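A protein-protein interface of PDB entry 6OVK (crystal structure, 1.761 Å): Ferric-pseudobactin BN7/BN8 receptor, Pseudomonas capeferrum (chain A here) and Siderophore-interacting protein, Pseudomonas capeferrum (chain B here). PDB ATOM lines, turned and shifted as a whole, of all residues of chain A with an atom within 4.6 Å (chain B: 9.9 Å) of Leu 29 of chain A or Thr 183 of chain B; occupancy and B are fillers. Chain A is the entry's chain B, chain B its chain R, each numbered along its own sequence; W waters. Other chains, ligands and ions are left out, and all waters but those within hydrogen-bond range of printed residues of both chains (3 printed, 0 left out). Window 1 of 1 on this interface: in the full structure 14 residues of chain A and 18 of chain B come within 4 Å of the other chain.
The backbone NH of Ser 30 of chain A lies within hydrogen-bond range of the backbone carbonyl oxygen of Tyr 73 of chain A. The backbone carbonyl oxygen (O) of Ala 19 of chain A sits close to the side-chain amide oxygen (OE1) of Gln 23 of chain A, at 3.1 Å. The backbone carbonyl oxygen (O) of Gly 182 of chain B sits at hydrogen-bond distance from the backbone NH (N) of Ala 149 of chain B (2.9 Å). The backbone NH of Met 146 of chain B lies within hydrogen-bond range of the backbone carbonyl oxygen of Ala 141 of chain B (3.1 Å). O of Ala 195 of chain B is in hydrogen-bond range of OG1 of Thr 199 of chain B, at 3.2 Å. The backbone carbonyl oxygen (O) of Ser 30 of chain A is in hydrogen-bond range of the side-chain hydroxyl (OG) of Ser 74 of chain A, 3.0 Å away.
Water W3 lies within hydrogen-bond range of the side-chain hydroxyl (OG) of Ser 74 of chain A (2.5 Å), the side-chain hydroxyl (OG1) of Thr 199 of chain B (2.8 Å) and the backbone carbonyl oxygen (O) of Ser 30 of chain A (3.1 Å). Water W1 lies within hydrogen-bond range of OG of Ser 30 of chain A and O of Ser 181 of chain B. Water W2 lies within hydrogen-bond range of the backbone carbonyl oxygen of Tyr 31 of chain A and the backbone NH of Ser 181 of chain B.
Leu 18 of chain A touches none of the printed residues of chain B. Of chain B, only Val 148 (3.7 Å), Gln 150 (3.7 Å) and Thr 183 (3.6 Å) come within 4 Å of Ala 19 of chain A. Of chain B, only Thr 183, Phe 184, Pro 185, Lys 191 and Ala 195 come within 4 Å of Leu 28 of chain A. Leu 29 of chain A touches just these residues of chain B: Gly 182 and Thr 183. Ser 30 of chain A touches just these residues of chain B: Ser 181 (3.8 Å), Ala 195 (3.5 Å) and Thr 199 (2.6 Å). Of the printed residues of chain A, Ser 181 of chain B touches Ser 30 (3.8 Å) and Tyr 31 (3.5 Å). Of the printed residues of chain A, Ala 195 of chain B touches Leu 28 and Ser 30. The nearest printed residue of chain B that does not touch Leu 29 of chain A is Phe 184 of chain B (4.1 Å). The nearest printed residue of chain A that does not touch Met 146 of chain B is Gln 23 of chain A (4.3 Å).
CG1 of Val 148 of chain B touches CB of Ala 19 of chain A, 3.7 Å away. Gln 150 of chain B touches Ala 19 of chain A (CD to CB, 3.7 Å). CB of Ala 141 of chain B touches NE2 of Gln 23 of chain A, 3.7 Å away. Thr 183 of chain B touches Gln 23 of chain A. Leu 28 of chain A touches Pro 185 of chain B (CA to CD, 3.5 Å). Leu 28 of chain A touches Lys 191 of chain B (CD1 to O, 3.6 Å). CB of Ala 195 of chain B touches CD2 of Leu 28 of chain A, at 3.6 Å. O of Leu 29 of chain A touches CA of Gly 182 of chain B, 2.9 Å away. Ser 181 of chain B touches Ser 30 of chain A (O to CA, 3.8 Å). CG2 of Thr 199 of chain B touches C of Tyr 31 of chain A, at 3.4 Å.
Of the 13 printed residues of chain A, 8 touch a printed residue of chain B. Printed residues of chain A that touch a printed residue of chain B: Ala 19, Gly 22, Gln 23, Ile 27, Leu 28, Leu 29, Ser 30 and Tyr 31. Hydrophobic or aromatic side chains of chain A within 4 Å of the printed part of chain B: Ala 19, Leu 28, Leu 29 and Tyr 31. Of the 26 printed residues of chain B, 12 touch a printed residue of chain A. Hydrophobic or aromatic side chains of chain B within 4 Å of the printed part of chain A: Ala 141, Met 146, Val 148, Phe 184, Pro 185 and Ala 195.
O of Leu 29 of chain A sits at hydrogen-bond distance from N of Thr 183 of chain B (2.9 Å). The backbone carbonyl oxygen (O) of Ile 27 of chain A is in hydrogen-bond range of the side-chain hydroxyl (OG1) of Thr 183 of chain B (2.9 Å). The backbone carbonyl oxygen (O) of Ser 181 of chain B is in hydrogen-bond range of the backbone NH (N) of Tyr 31 of chain A (3.5 Å). The side-chain hydroxyl of Thr 199 of chain B is in hydrogen-bond range of the side-chain hydroxyl of Ser 30 of chain A, 2.6 Å away.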
ATOM      1  N   LEU A  18     -11.097  -5.557  35.307  1.00  0.00           N
ATOM      2  CA  LEU A  18     -10.196  -6.000  34.244  1.00  0.00           C
ATOM      3  C   LEU A  18     -10.932  -6.105  32.911  1.00  0.00           C
ATOM      4  O   LEU A  18     -10.328  -5.876  31.860  1.00  0.00           O
ATOM      5  CB  LEU A  18      -9.597  -7.364  34.588  1.00  0.00           C
ATOM      6  CG  LEU A  18      -8.537  -7.403  35.683  1.00  0.00           C
ATOM      7  CD1 LEU A  18      -8.382  -8.839  36.120  1.00  0.00           C
ATOM      8  CD2 LEU A  18      -7.208  -6.815  35.141  1.00  0.00           C
ATOM      9  N   ALA A  19     -12.219  -6.439  32.933  1.00  0.00           N
ATOM     10  CA  ALA A  19     -13.001  -6.364  31.702  1.00  0.00           C
ATOM     11  C   ALA A  19     -13.012  -4.938  31.164  1.00  0.00           C
ATOM     12  O   ALA A  19     -12.855  -4.698  29.953  1.00  0.00           O
ATOM     13  CB  ALA A  19     -14.423  -6.839  31.988  1.00  0.00           C
ATOM     14  N   GLY A  22      -9.366  -3.979  29.877  1.00  0.00           N
ATOM     15  CA  GLY A  22      -8.909  -4.515  28.613  1.00  0.00           C
ATOM     16  C   GLY A  22      -9.656  -3.882  27.467  1.00  0.00           C
ATOM     17  O   GLY A  22      -9.097  -3.693  26.374  1.00  0.00           O
ATOM     18  N   GLN A  23     -10.898  -3.466  27.723  1.00  0.00           N
ATOM     19  CA  GLN A  23     -11.614  -2.689  26.717  1.00  0.00           C
ATOM     20  C   GLN A  23     -11.048  -1.280  26.561  1.00  0.00           C
ATOM     21  O   GLN A  23     -10.884  -0.806  25.432  1.00  0.00           O
ATOM     22  CB  GLN A  23     -13.080  -2.622  27.074  1.00  0.00           C
ATOM     23  CG  GLN A  23     -13.733  -3.894  26.936  1.00  0.00           C
ATOM     24  CD  GLN A  23     -15.171  -3.809  27.361  1.00  0.00           C
ATOM     25  OE1 GLN A  23     -15.519  -4.097  28.524  1.00  0.00           O
ATOM     26  NE2 GLN A  23     -16.021  -3.401  26.428  1.00  0.00           N
ATOM     27  N   ILE A  27      -6.796  -4.277  24.253  1.00  0.00           N
ATOM     28  CA  ILE A  27      -5.713  -5.255  24.265  1.00  0.00           C
ATOM     29  C   ILE A  27      -6.293  -6.658  24.363  1.00  0.00           C
ATOM     30  O   ILE A  27      -7.448  -6.858  24.765  1.00  0.00           O
ATOM     31  CB  ILE A  27      -4.716  -5.048  25.419  1.00  0.00           C
ATOM     32  CG1 ILE A  27      -5.473  -5.029  26.761  1.00  0.00           C
ATOM     33  CG2 ILE A  27      -3.927  -3.774  25.217  1.00  0.00           C
ATOM     34  CD1 ILE A  27      -4.511  -5.117  27.982  1.00  0.00           C
ATOM     35  N   LEU A  28      -5.485  -7.625  23.923  1.00  0.00           N
ATOM     36  CA  LEU A  28      -5.781  -9.041  24.113  1.00  0.00           C
ATOM     37  C   LEU A  28      -5.232  -9.406  25.482  1.00  0.00           C
ATOM     38  O   LEU A  28      -4.014  -9.523  25.668  1.00  0.00           O
ATOM     39  CB  LEU A  28      -5.183  -9.908  22.995  1.00  0.00           C
ATOM     40  CG  LEU A  28      -5.867 -11.295  22.783  1.00  0.00           C
ATOM     41  CD1 LEU A  28      -5.128 -12.064  21.735  1.00  0.00           C
ATOM     42  CD2 LEU A  28      -5.868 -12.150  24.075  1.00  0.00           C
ATOM     43  N   LEU A  29      -6.134  -9.568  26.441  1.00  0.00           N
ATOM     44  CA  LEU A  29      -5.803  -9.915  27.811  1.00  0.00           C
ATOM     45  C   LEU A  29      -6.511 -11.221  28.125  1.00  0.00           C
ATOM     46  O   LEU A  29      -7.726 -11.320  27.926  1.00  0.00           O
ATOM     47  CB  LEU A  29      -6.282  -8.803  28.738  1.00  0.00           C
ATOM     48  CG  LEU A  29      -6.250  -8.977  30.250  1.00  0.00           C
ATOM     49  CD1 LEU A  29      -4.806  -9.150  30.780  1.00  0.00           C
ATOM     50  CD2 LEU A  29      -6.880  -7.736  30.870  1.00  0.00           C
ATOM     51  N   SER A  30      -5.760 -12.248  28.524  1.00  0.00           N
ATOM     52  CA  SER A  30      -6.358 -13.562  28.741  1.00  0.00           C
ATOM     53  C   SER A  30      -5.695 -14.196  29.955  1.00  0.00           C
ATOM     54  O   SER A  30      -4.468 -14.231  29.996  1.00  0.00           O
ATOM     55  CB  SER A  30      -6.154 -14.437  27.488  1.00  0.00           C
ATOM     56  OG  SER A  30      -6.504 -15.772  27.702  1.00  0.00           O
ATOM     57  N   TYR A  31      -6.483 -14.689  30.919  1.00  0.00           N
ATOM     58  CA  TYR A  31      -5.933 -15.227  32.163  1.00  0.00           C
ATOM     59  C   TYR A  31      -6.972 -16.159  32.782  1.00  0.00           C
ATOM     60  O   TYR A  31      -8.149 -16.117  32.415  1.00  0.00           O
ATOM     61  CB  TYR A  31      -5.583 -14.088  33.144  1.00  0.00           C
ATOM     62  CG  TYR A  31      -6.751 -13.170  33.272  1.00  0.00           C
ATOM     63  CD1 TYR A  31      -7.750 -13.414  34.184  1.00  0.00           C
ATOM     64  CD2 TYR A  31      -6.887 -12.078  32.417  1.00  0.00           C
ATOM     65  CE1 TYR A  31      -8.865 -12.605  34.252  1.00  0.00           C
ATOM     66  CE2 TYR A  31      -7.975 -11.259  32.483  1.00  0.00           C
ATOM     67  CZ  TYR A  31      -8.966 -11.517  33.401  1.00  0.00           C
ATOM     68  OH  TYR A  31     -10.036 -10.656  33.431  1.00  0.00           O
ATOM     69  N   LEU A  54      -1.825  -1.312  34.181  1.00  0.00           N
ATOM     70  CA  LEU A  54      -2.259  -2.621  34.641  1.00  0.00           C
ATOM     71  C   LEU A  54      -1.638  -2.944  35.997  1.00  0.00           C
ATOM     72  O   LEU A  54      -2.335  -3.401  36.906  1.00  0.00           O
ATOM     73  CB  LEU A  54      -1.943  -3.679  33.565  1.00  0.00           C
ATOM     74  CG  LEU A  54      -2.410  -5.118  33.804  1.00  0.00           C
ATOM     75  CD1 LEU A  54      -3.906  -5.133  34.204  1.00  0.00           C
ATOM     76  CD2 LEU A  54      -2.187  -5.986  32.594  1.00  0.00           C
ATOM     77  N   TYR A  73      -1.523 -10.068  26.629  1.00  0.00           N
ATOM     78  CA  TYR A  73      -1.248  -9.946  28.052  1.00  0.00           C
ATOM     79  C   TYR A  73      -1.908 -11.084  28.810  1.00  0.00           C
ATOM     80  O   TYR A  73      -2.965 -11.567  28.424  1.00  0.00           O
ATOM     81  CB  TYR A  73      -1.788  -8.631  28.608  1.00  0.00           C
ATOM     82  CG  TYR A  73      -1.218  -7.377  27.991  1.00  0.00           C
ATOM     83  CD1 TYR A  73      -1.576  -6.992  26.717  1.00  0.00           C
ATOM     84  CD2 TYR A  73      -0.359  -6.545  28.717  1.00  0.00           C
ATOM     85  CE1 TYR A  73      -1.076  -5.828  26.149  1.00  0.00           C
ATOM     86  CE2 TYR A  73       0.142  -5.373  28.149  1.00  0.00           C
ATOM     87  CZ  TYR A  73      -0.221  -5.027  26.870  1.00  0.00           C
ATOM     88  OH  TYR A  73       0.243  -3.877  26.270  1.00  0.00           O
ATOM     89  N   SER A  74      -1.290 -11.470  29.919  1.00  0.00           N
ATOM     90  CA  SER A  74      -1.855 -12.391  30.887  1.00  0.00           C
ATOM     91  C   SER A  74      -1.634 -11.833  32.297  1.00  0.00           C
ATOM     92  O   SER A  74      -1.171 -10.708  32.476  1.00  0.00           O
ATOM     93  CB  SER A  74      -1.215 -13.769  30.749  1.00  0.00           C
ATOM     94  OG  SER A  74      -1.902 -14.706  31.533  1.00  0.00           O
ATOM     95  N   LEU A  75      -2.043 -12.607  33.287  1.00  0.00           N
ATOM     96  CA  LEU A  75      -1.891 -12.264  34.700  1.00  0.00           C
ATOM     97  C   LEU A  75      -1.306 -13.460  35.408  1.00  0.00           C
ATOM     98  O   LEU A  75      -1.591 -14.601  35.039  1.00  0.00           O
ATOM     99  CB  LEU A  75      -3.256 -11.941  35.360  1.00  0.00           C
ATOM    100  CG  LEU A  75      -3.960 -10.759  34.742  1.00  0.00           C
ATOM    101  CD1 LEU A  75      -5.225 -10.490  35.536  1.00  0.00           C
ATOM    102  CD2 LEU A  75      -3.008  -9.554  34.754  1.00  0.00           C
ATOM    103  N   ALA B 141     -19.400  -4.762  23.697  1.00  0.00           N
ATOM    104  CA  ALA B 141     -17.986  -4.818  23.361  1.00  0.00           C
ATOM    105  C   ALA B 141     -17.774  -4.932  21.858  1.00  0.00           C
ATOM    106  O   ALA B 141     -16.856  -4.303  21.328  1.00  0.00           O
ATOM    107  CB  ALA B 141     -17.296  -5.962  24.117  1.00  0.00           C
ATOM    108  N   GLN B 144     -17.094  -1.827  19.775  1.00  0.00           N
ATOM    109  CA  GLN B 144     -15.776  -1.234  19.811  1.00  0.00           C
ATOM    110  C   GLN B 144     -14.714  -2.221  19.349  1.00  0.00           C
ATOM    111  O   GLN B 144     -13.533  -2.041  19.665  1.00  0.00           O
ATOM    112  CB  GLN B 144     -15.475  -0.712  21.213  1.00  0.00           C
ATOM    113  CG  GLN B 144     -16.439   0.407  21.567  1.00  0.00           C
ATOM    114  CD  GLN B 144     -16.595   0.648  23.034  1.00  0.00           C
ATOM    115  OE1 GLN B 144     -15.945   0.005  23.872  1.00  0.00           O
ATOM    116  NE2 GLN B 144     -17.492   1.578  23.371  1.00  0.00           N
ATOM    117  N   GLY B 145     -15.118  -3.248  18.607  1.00  0.00           N
ATOM    118  CA  GLY B 145     -14.174  -4.176  18.044  1.00  0.00           C
ATOM    119  C   GLY B 145     -13.620  -5.196  19.009  1.00  0.00           C
ATOM    120  O   GLY B 145     -12.509  -5.677  18.803  1.00  0.00           O
ATOM    121  N   MET B 146     -14.321  -5.497  20.092  1.00  0.00           N
ATOM    122  CA  MET B 146     -13.805  -6.438  21.089  1.00  0.00           C
ATOM    123  C   MET B 146     -14.819  -7.519  21.438  1.00  0.00           C
ATOM    124  O   MET B 146     -16.040  -7.297  21.376  1.00  0.00           O
ATOM    125  CB  MET B 146     -13.442  -5.678  22.400  1.00  0.00           C
ATOM    126  CG  MET B 146     -12.545  -4.480  22.221  1.00  0.00           C
ATOM    127  SD  MET B 146     -10.831  -5.038  22.166  1.00  0.00           S
ATOM    128  CE  MET B 146     -10.560  -5.723  23.792  1.00  0.00           C
ATOM    129  N   LEU B 147     -14.323  -8.672  21.899  1.00  0.00           N
ATOM    130  CA  LEU B 147     -15.124  -9.607  22.690  1.00  0.00           C
ATOM    131  C   LEU B 147     -14.645  -9.503  24.129  1.00  0.00           C
ATOM    132  O   LEU B 147     -13.446  -9.348  24.368  1.00  0.00           O
ATOM    133  CB  LEU B 147     -14.959 -11.072  22.254  1.00  0.00           C
ATOM    134  CG  LEU B 147     -15.359 -11.502  20.859  1.00  0.00           C
ATOM    135  CD1 LEU B 147     -15.253 -13.008  20.775  1.00  0.00           C
ATOM    136  CD2 LEU B 147     -16.750 -11.028  20.586  1.00  0.00           C
ATOM    137  N   VAL B 148     -15.568  -9.616  25.092  1.00  0.00           N
ATOM    138  CA  VAL B 148     -15.202  -9.531  26.515  1.00  0.00           C
ATOM    139  C   VAL B 148     -15.833 -10.731  27.195  1.00  0.00           C
ATOM    140  O   VAL B 148     -17.010 -11.040  26.954  1.00  0.00           O
ATOM    141  CB  VAL B 148     -15.683  -8.224  27.155  1.00  0.00           C
ATOM    142  CG1 VAL B 148     -15.466  -8.210  28.696  1.00  0.00           C
ATOM    143  CG2 VAL B 148     -14.927  -7.081  26.499  1.00  0.00           C
ATOM    144  N   ALA B 149     -15.049 -11.452  27.975  1.00  0.00           N
ATOM    145  CA  ALA B 149     -15.569 -12.653  28.627  1.00  0.00           C
ATOM    146  C   ALA B 149     -15.258 -12.565  30.101  1.00  0.00           C
ATOM    147  O   ALA B 149     -14.139 -12.192  30.472  1.00  0.00           O
ATOM    148  CB  ALA B 149     -14.947 -13.922  28.035  1.00  0.00           C
ATOM    149  N   GLN B 150     -16.273 -12.819  30.935  1.00  0.00           N
ATOM    150  CA  GLN B 150     -16.135 -12.706  32.384  1.00  0.00           C
ATOM    151  C   GLN B 150     -16.600 -14.049  32.947  1.00  0.00           C
ATOM    152  O   GLN B 150     -17.746 -14.198  33.391  1.00  0.00           O
ATOM    153  CB  GLN B 150     -16.955 -11.508  32.903  1.00  0.00           C
ATOM    154  CG  GLN B 150     -16.555 -10.217  32.144  1.00  0.00           C
ATOM    155  CD  GLN B 150     -17.374  -8.991  32.506  1.00  0.00           C
ATOM    156  OE1 GLN B 150     -17.975  -8.347  31.639  1.00  0.00           O
ATOM    157  NE2 GLN B 150     -17.384  -8.660  33.770  1.00  0.00           N
ATOM    158  N   GLY B 151     -15.699 -15.023  32.941  1.00  0.00           N
ATOM    159  CA  GLY B 151     -16.062 -16.335  33.416  1.00  0.00           C
ATOM    160  C   GLY B 151     -17.041 -17.031  32.508  1.00  0.00           C
ATOM    161  O   GLY B 151     -17.858 -17.854  32.975  1.00  0.00           O
ATOM    162  N   GLN B 152     -16.972 -16.743  31.201  1.00  0.00           N
ATOM    163  CA  GLN B 152     -17.957 -17.319  30.294  1.00  0.00           C
ATOM    164  C   GLN B 152     -17.613 -18.777  30.000  1.00  0.00           C
ATOM    165  O   GLN B 152     -16.467 -19.074  29.657  1.00  0.00           O
ATOM    166  CB  GLN B 152     -17.994 -16.517  28.984  1.00  0.00           C
ATOM    167  CG  GLN B 152     -19.113 -16.979  28.002  1.00  0.00           C
ATOM    168  CD  GLN B 152     -19.203 -16.149  26.763  1.00  0.00           C
ATOM    169  OE1 GLN B 152     -18.237 -15.521  26.341  1.00  0.00           O
ATOM    170  NE2 GLN B 152     -20.400 -16.147  26.143  1.00  0.00           N
ATOM    171  N   PHE B 157     -18.545 -19.182  24.799  1.00  0.00           N
ATOM    172  CA  PHE B 157     -17.578 -18.252  24.239  1.00  0.00           C
ATOM    173  C   PHE B 157     -17.273 -18.599  22.791  1.00  0.00           C
ATOM    174  O   PHE B 157     -17.225 -17.729  21.917  1.00  0.00           O
ATOM    175  CB  PHE B 157     -16.303 -18.296  25.077  1.00  0.00           C
ATOM    176  CG  PHE B 157     -15.228 -17.405  24.543  1.00  0.00           C
ATOM    177  CD1 PHE B 157     -15.278 -16.038  24.778  1.00  0.00           C
ATOM    178  CD2 PHE B 157     -14.191 -17.929  23.772  1.00  0.00           C
ATOM    179  CE1 PHE B 157     -14.248 -15.187  24.267  1.00  0.00           C
ATOM    180  CE2 PHE B 157     -13.170 -17.118  23.257  1.00  0.00           C
ATOM    181  CZ  PHE B 157     -13.199 -15.732  23.479  1.00  0.00           C
ATOM    182  N   VAL B 180     -13.923 -18.822  30.646  1.00  0.00           N
ATOM    183  CA  VAL B 180     -13.060 -17.933  29.860  1.00  0.00           C
ATOM    184  C   VAL B 180     -13.153 -16.523  30.414  1.00  0.00           C
ATOM    185  O   VAL B 180     -14.260 -15.978  30.559  1.00  0.00           O
ATOM    186  CB  VAL B 180     -13.468 -17.942  28.383  1.00  0.00           C
ATOM    187  CG1 VAL B 180     -12.563 -16.982  27.597  1.00  0.00           C
ATOM    188  CG2 VAL B 180     -13.333 -19.363  27.869  1.00  0.00           C
ATOM    189  N   SER B 181     -12.001 -15.920  30.714  1.00  0.00           N
ATOM    190  CA  SER B 181     -11.941 -14.513  31.118  1.00  0.00           C
ATOM    191  C   SER B 181     -10.946 -13.767  30.242  1.00  0.00           C
ATOM    192  O   SER B 181      -9.815 -14.229  30.039  1.00  0.00           O
ATOM    193  CB  SER B 181     -11.539 -14.366  32.586  1.00  0.00           C
ATOM    194  OG  SER B 181     -12.635 -14.791  33.391  1.00  0.00           O
ATOM    195  N   GLY B 182     -11.340 -12.602  29.765  1.00  0.00           N
ATOM    196  CA  GLY B 182     -10.360 -11.769  29.089  1.00  0.00           C
ATOM    197  C   GLY B 182     -11.047 -10.781  28.183  1.00  0.00           C
ATOM    198  O   GLY B 182     -12.261 -10.675  28.170  1.00  0.00           O
ATOM    199  N   THR B 183     -10.219 -10.022  27.454  1.00  0.00           N
ATOM    200  CA  THR B 183     -10.721  -9.107  26.433  1.00  0.00           C
ATOM    201  C   THR B 183      -9.992  -9.445  25.141  1.00  0.00           C
ATOM    202  O   THR B 183      -8.796  -9.768  25.158  1.00  0.00           O
ATOM    203  CB  THR B 183     -10.522  -7.636  26.827  1.00  0.00           C
ATOM    204  OG1 THR B 183      -9.125  -7.378  27.033  1.00  0.00           O
ATOM    205  CG2 THR B 183     -11.250  -7.319  28.110  1.00  0.00           C
ATOM    206  N   PHE B 184     -10.708  -9.346  24.005  1.00  0.00           N
ATOM    207  CA  PHE B 184     -10.185  -9.980  22.799  1.00  0.00           C
ATOM    208  C   PHE B 184     -10.457  -9.107  21.598  1.00  0.00           C
ATOM    209  O   PHE B 184     -11.623  -8.964  21.208  1.00  0.00           O
ATOM    210  CB  PHE B 184     -10.857 -11.327  22.621  1.00  0.00           C
ATOM    211  CG  PHE B 184     -10.645 -12.241  23.805  1.00  0.00           C
ATOM    212  CD1 PHE B 184      -9.471 -12.949  23.913  1.00  0.00           C
ATOM    213  CD2 PHE B 184     -11.626 -12.408  24.765  1.00  0.00           C
ATOM    214  CE1 PHE B 184      -9.282 -13.816  24.981  1.00  0.00           C
ATOM    215  CE2 PHE B 184     -11.428 -13.246  25.851  1.00  0.00           C
ATOM    216  CZ  PHE B 184     -10.267 -13.942  25.958  1.00  0.00           C
ATOM    217  N   PRO B 185      -9.445  -8.464  21.044  1.00  0.00           N
ATOM    218  CA  PRO B 185      -9.682  -7.627  19.864  1.00  0.00           C
ATOM    219  C   PRO B 185     -10.163  -8.482  18.698  1.00  0.00           C
ATOM    220  O   PRO B 185      -9.568  -9.523  18.385  1.00  0.00           O
ATOM    221  CB  PRO B 185      -8.303  -7.011  19.580  1.00  0.00           C
ATOM    222  CG  PRO B 185      -7.604  -7.038  20.948  1.00  0.00           C
ATOM    223  CD  PRO B 185      -8.076  -8.302  21.595  1.00  0.00           C
ATOM    224  N   LEU B 186     -11.246  -8.027  18.036  1.00  0.00           N
ATOM    225  CA  LEU B 186     -11.820  -8.837  16.954  1.00  0.00           C
ATOM    226  C   LEU B 186     -10.988  -8.800  15.672  1.00  0.00           C
ATOM    227  O   LEU B 186     -11.278  -9.567  14.739  1.00  0.00           O
ATOM    228  CB  LEU B 186     -13.235  -8.352  16.670  1.00  0.00           C
ATOM    229  CG  LEU B 186     -14.198  -8.870  17.751  1.00  0.00           C
ATOM    230  CD1 LEU B 186     -15.484  -8.042  17.596  1.00  0.00           C
ATOM    231  CD2 LEU B 186     -14.508 -10.384  17.588  1.00  0.00           C
ATOM    232  N   GLU B 187      -9.965  -7.934  15.616  1.00  0.00           N
ATOM    233  CA  GLU B 187      -9.112  -7.781  14.436  1.00  0.00           C
ATOM    234  C   GLU B 187      -8.415  -9.062  14.039  1.00  0.00           C
ATOM    235  O   GLU B 187      -8.057  -9.213  12.866  1.00  0.00           O
ATOM    236  CB  GLU B 187      -8.035  -6.709  14.678  1.00  0.00           C
ATOM    237  CG  GLU B 187      -8.580  -5.330  14.907  1.00  0.00           C
ATOM    238  CD  GLU B 187      -8.635  -4.956  16.390  1.00  0.00           C
ATOM    239  OE1 GLU B 187      -7.713  -4.240  16.851  1.00  0.00           O
ATOM    240  OE2 GLU B 187      -9.596  -5.396  17.077  1.00  0.00           O
ATOM    241  N   ASN B 188      -8.210  -9.998  14.966  1.00  0.00           N
ATOM    242  CA  ASN B 188      -7.524 -11.236  14.587  1.00  0.00           C
ATOM    243  C   ASN B 188      -8.105 -12.370  15.414  1.00  0.00           C
ATOM    244  O   ASN B 188      -7.737 -12.536  16.583  1.00  0.00           O
ATOM    245  CB  ASN B 188      -6.024 -11.096  14.805  1.00  0.00           C
ATOM    246  CG  ASN B 188      -5.267 -12.270  14.299  1.00  0.00           C
ATOM    247  OD1 ASN B 188      -5.709 -13.400  14.427  1.00  0.00           O
ATOM    248  ND2 ASN B 188      -4.102 -12.008  13.668  1.00  0.00           N
ATOM    249  N   LYS B 191      -5.683 -15.135  16.764  1.00  0.00           N
ATOM    250  CA  LYS B 191      -4.966 -14.804  17.997  1.00  0.00           C
ATOM    251  C   LYS B 191      -5.814 -15.062  19.226  1.00  0.00           C
ATOM    252  O   LYS B 191      -5.262 -15.401  20.294  1.00  0.00           O
ATOM    253  CB  LYS B 191      -4.512 -13.344  17.945  1.00  0.00           C
ATOM    254  CG  LYS B 191      -3.284 -13.161  17.073  1.00  0.00           C
ATOM    255  CD  LYS B 191      -2.896 -11.671  17.044  1.00  0.00           C
ATOM    256  CE  LYS B 191      -1.671 -11.399  16.191  1.00  0.00           C
ATOM    257  NZ  LYS B 191      -1.124 -10.027  16.529  1.00  0.00           N
ATOM    258  N   ILE B 192      -7.136 -14.814  19.125  1.00  0.00           N
ATOM    259  CA  ILE B 192      -8.067 -15.098  20.224  1.00  0.00           C
ATOM    260  C   ILE B 192      -8.048 -16.586  20.569  1.00  0.00           C
ATOM    261  O   ILE B 192      -7.869 -16.979  21.735  1.00  0.00           O
ATOM    262  CB  ILE B 192      -9.494 -14.658  19.846  1.00  0.00           C
ATOM    263  CG1 ILE B 192      -9.519 -13.142  19.514  1.00  0.00           C
ATOM    264  CG2 ILE B 192     -10.507 -15.068  20.996  1.00  0.00           C
ATOM    265  CD1 ILE B 192     -10.925 -12.660  19.082  1.00  0.00           C
ATOM    266  N   ILE B 193      -8.221 -17.429  19.554  1.00  0.00           N
ATOM    267  CA  ILE B 193      -8.187 -18.875  19.764  1.00  0.00           C
ATOM    268  C   ILE B 193      -6.888 -19.286  20.419  1.00  0.00           C
ATOM    269  O   ILE B 193      -6.881 -20.070  21.376  1.00  0.00           O
ATOM    270  CB  ILE B 193      -8.406 -19.611  18.425  1.00  0.00           C
ATOM    271  CG1 ILE B 193      -9.836 -19.348  17.934  1.00  0.00           C
ATOM    272  CG2 ILE B 193      -8.186 -21.124  18.570  1.00  0.00           C
ATOM    273  CD1 ILE B 193     -10.077 -19.795  16.474  1.00  0.00           C
ATOM    274  N   ALA B 195      -4.723 -17.570  22.193  1.00  0.00           N
ATOM    275  CA  ALA B 195      -4.573 -17.057  23.555  1.00  0.00           C
ATOM    276  C   ALA B 195      -5.454 -17.826  24.524  1.00  0.00           C
ATOM    277  O   ALA B 195      -4.997 -18.195  25.617  1.00  0.00           O
ATOM    278  CB  ALA B 195      -4.883 -15.543  23.603  1.00  0.00           C
ATOM    279  N   VAL B 196      -6.709 -18.088  24.146  1.00  0.00           N
ATOM    280  CA  VAL B 196      -7.599 -18.818  25.043  1.00  0.00           C
ATOM    281  C   VAL B 196      -7.099 -20.238  25.241  1.00  0.00           C
ATOM    282  O   VAL B 196      -7.127 -20.769  26.356  1.00  0.00           O
ATOM    283  CB  VAL B 196      -9.026 -18.766  24.501  1.00  0.00           C
ATOM    284  CG1 VAL B 196      -9.955 -19.717  25.285  1.00  0.00           C
ATOM    285  CG2 VAL B 196      -9.540 -17.308  24.602  1.00  0.00           C
ATOM    286  N   THR B 199      -4.116 -20.078  27.688  1.00  0.00           N
ATOM    287  CA  THR B 199      -4.550 -19.851  29.068  1.00  0.00           C
ATOM    288  C   THR B 199      -5.185 -21.095  29.674  1.00  0.00           C
ATOM    289  O   THR B 199      -4.906 -21.442  30.838  1.00  0.00           O
ATOM    290  CB  THR B 199      -5.513 -18.683  29.091  1.00  0.00           C
ATOM    291  OG1 THR B 199      -4.784 -17.516  28.691  1.00  0.00           O
ATOM    292  CG2 THR B 199      -6.141 -18.502  30.485  1.00  0.00           C
HETATM  293  O   HOH W   1      -8.979 -16.286  28.423  1.00  0.00           O
HETATM  294  O   HOH W   2      -9.646 -17.812  30.847  1.00  0.00           O
HETATM  295  O   HOH W   3      -2.787 -16.837  30.507  1.00  0.00           O
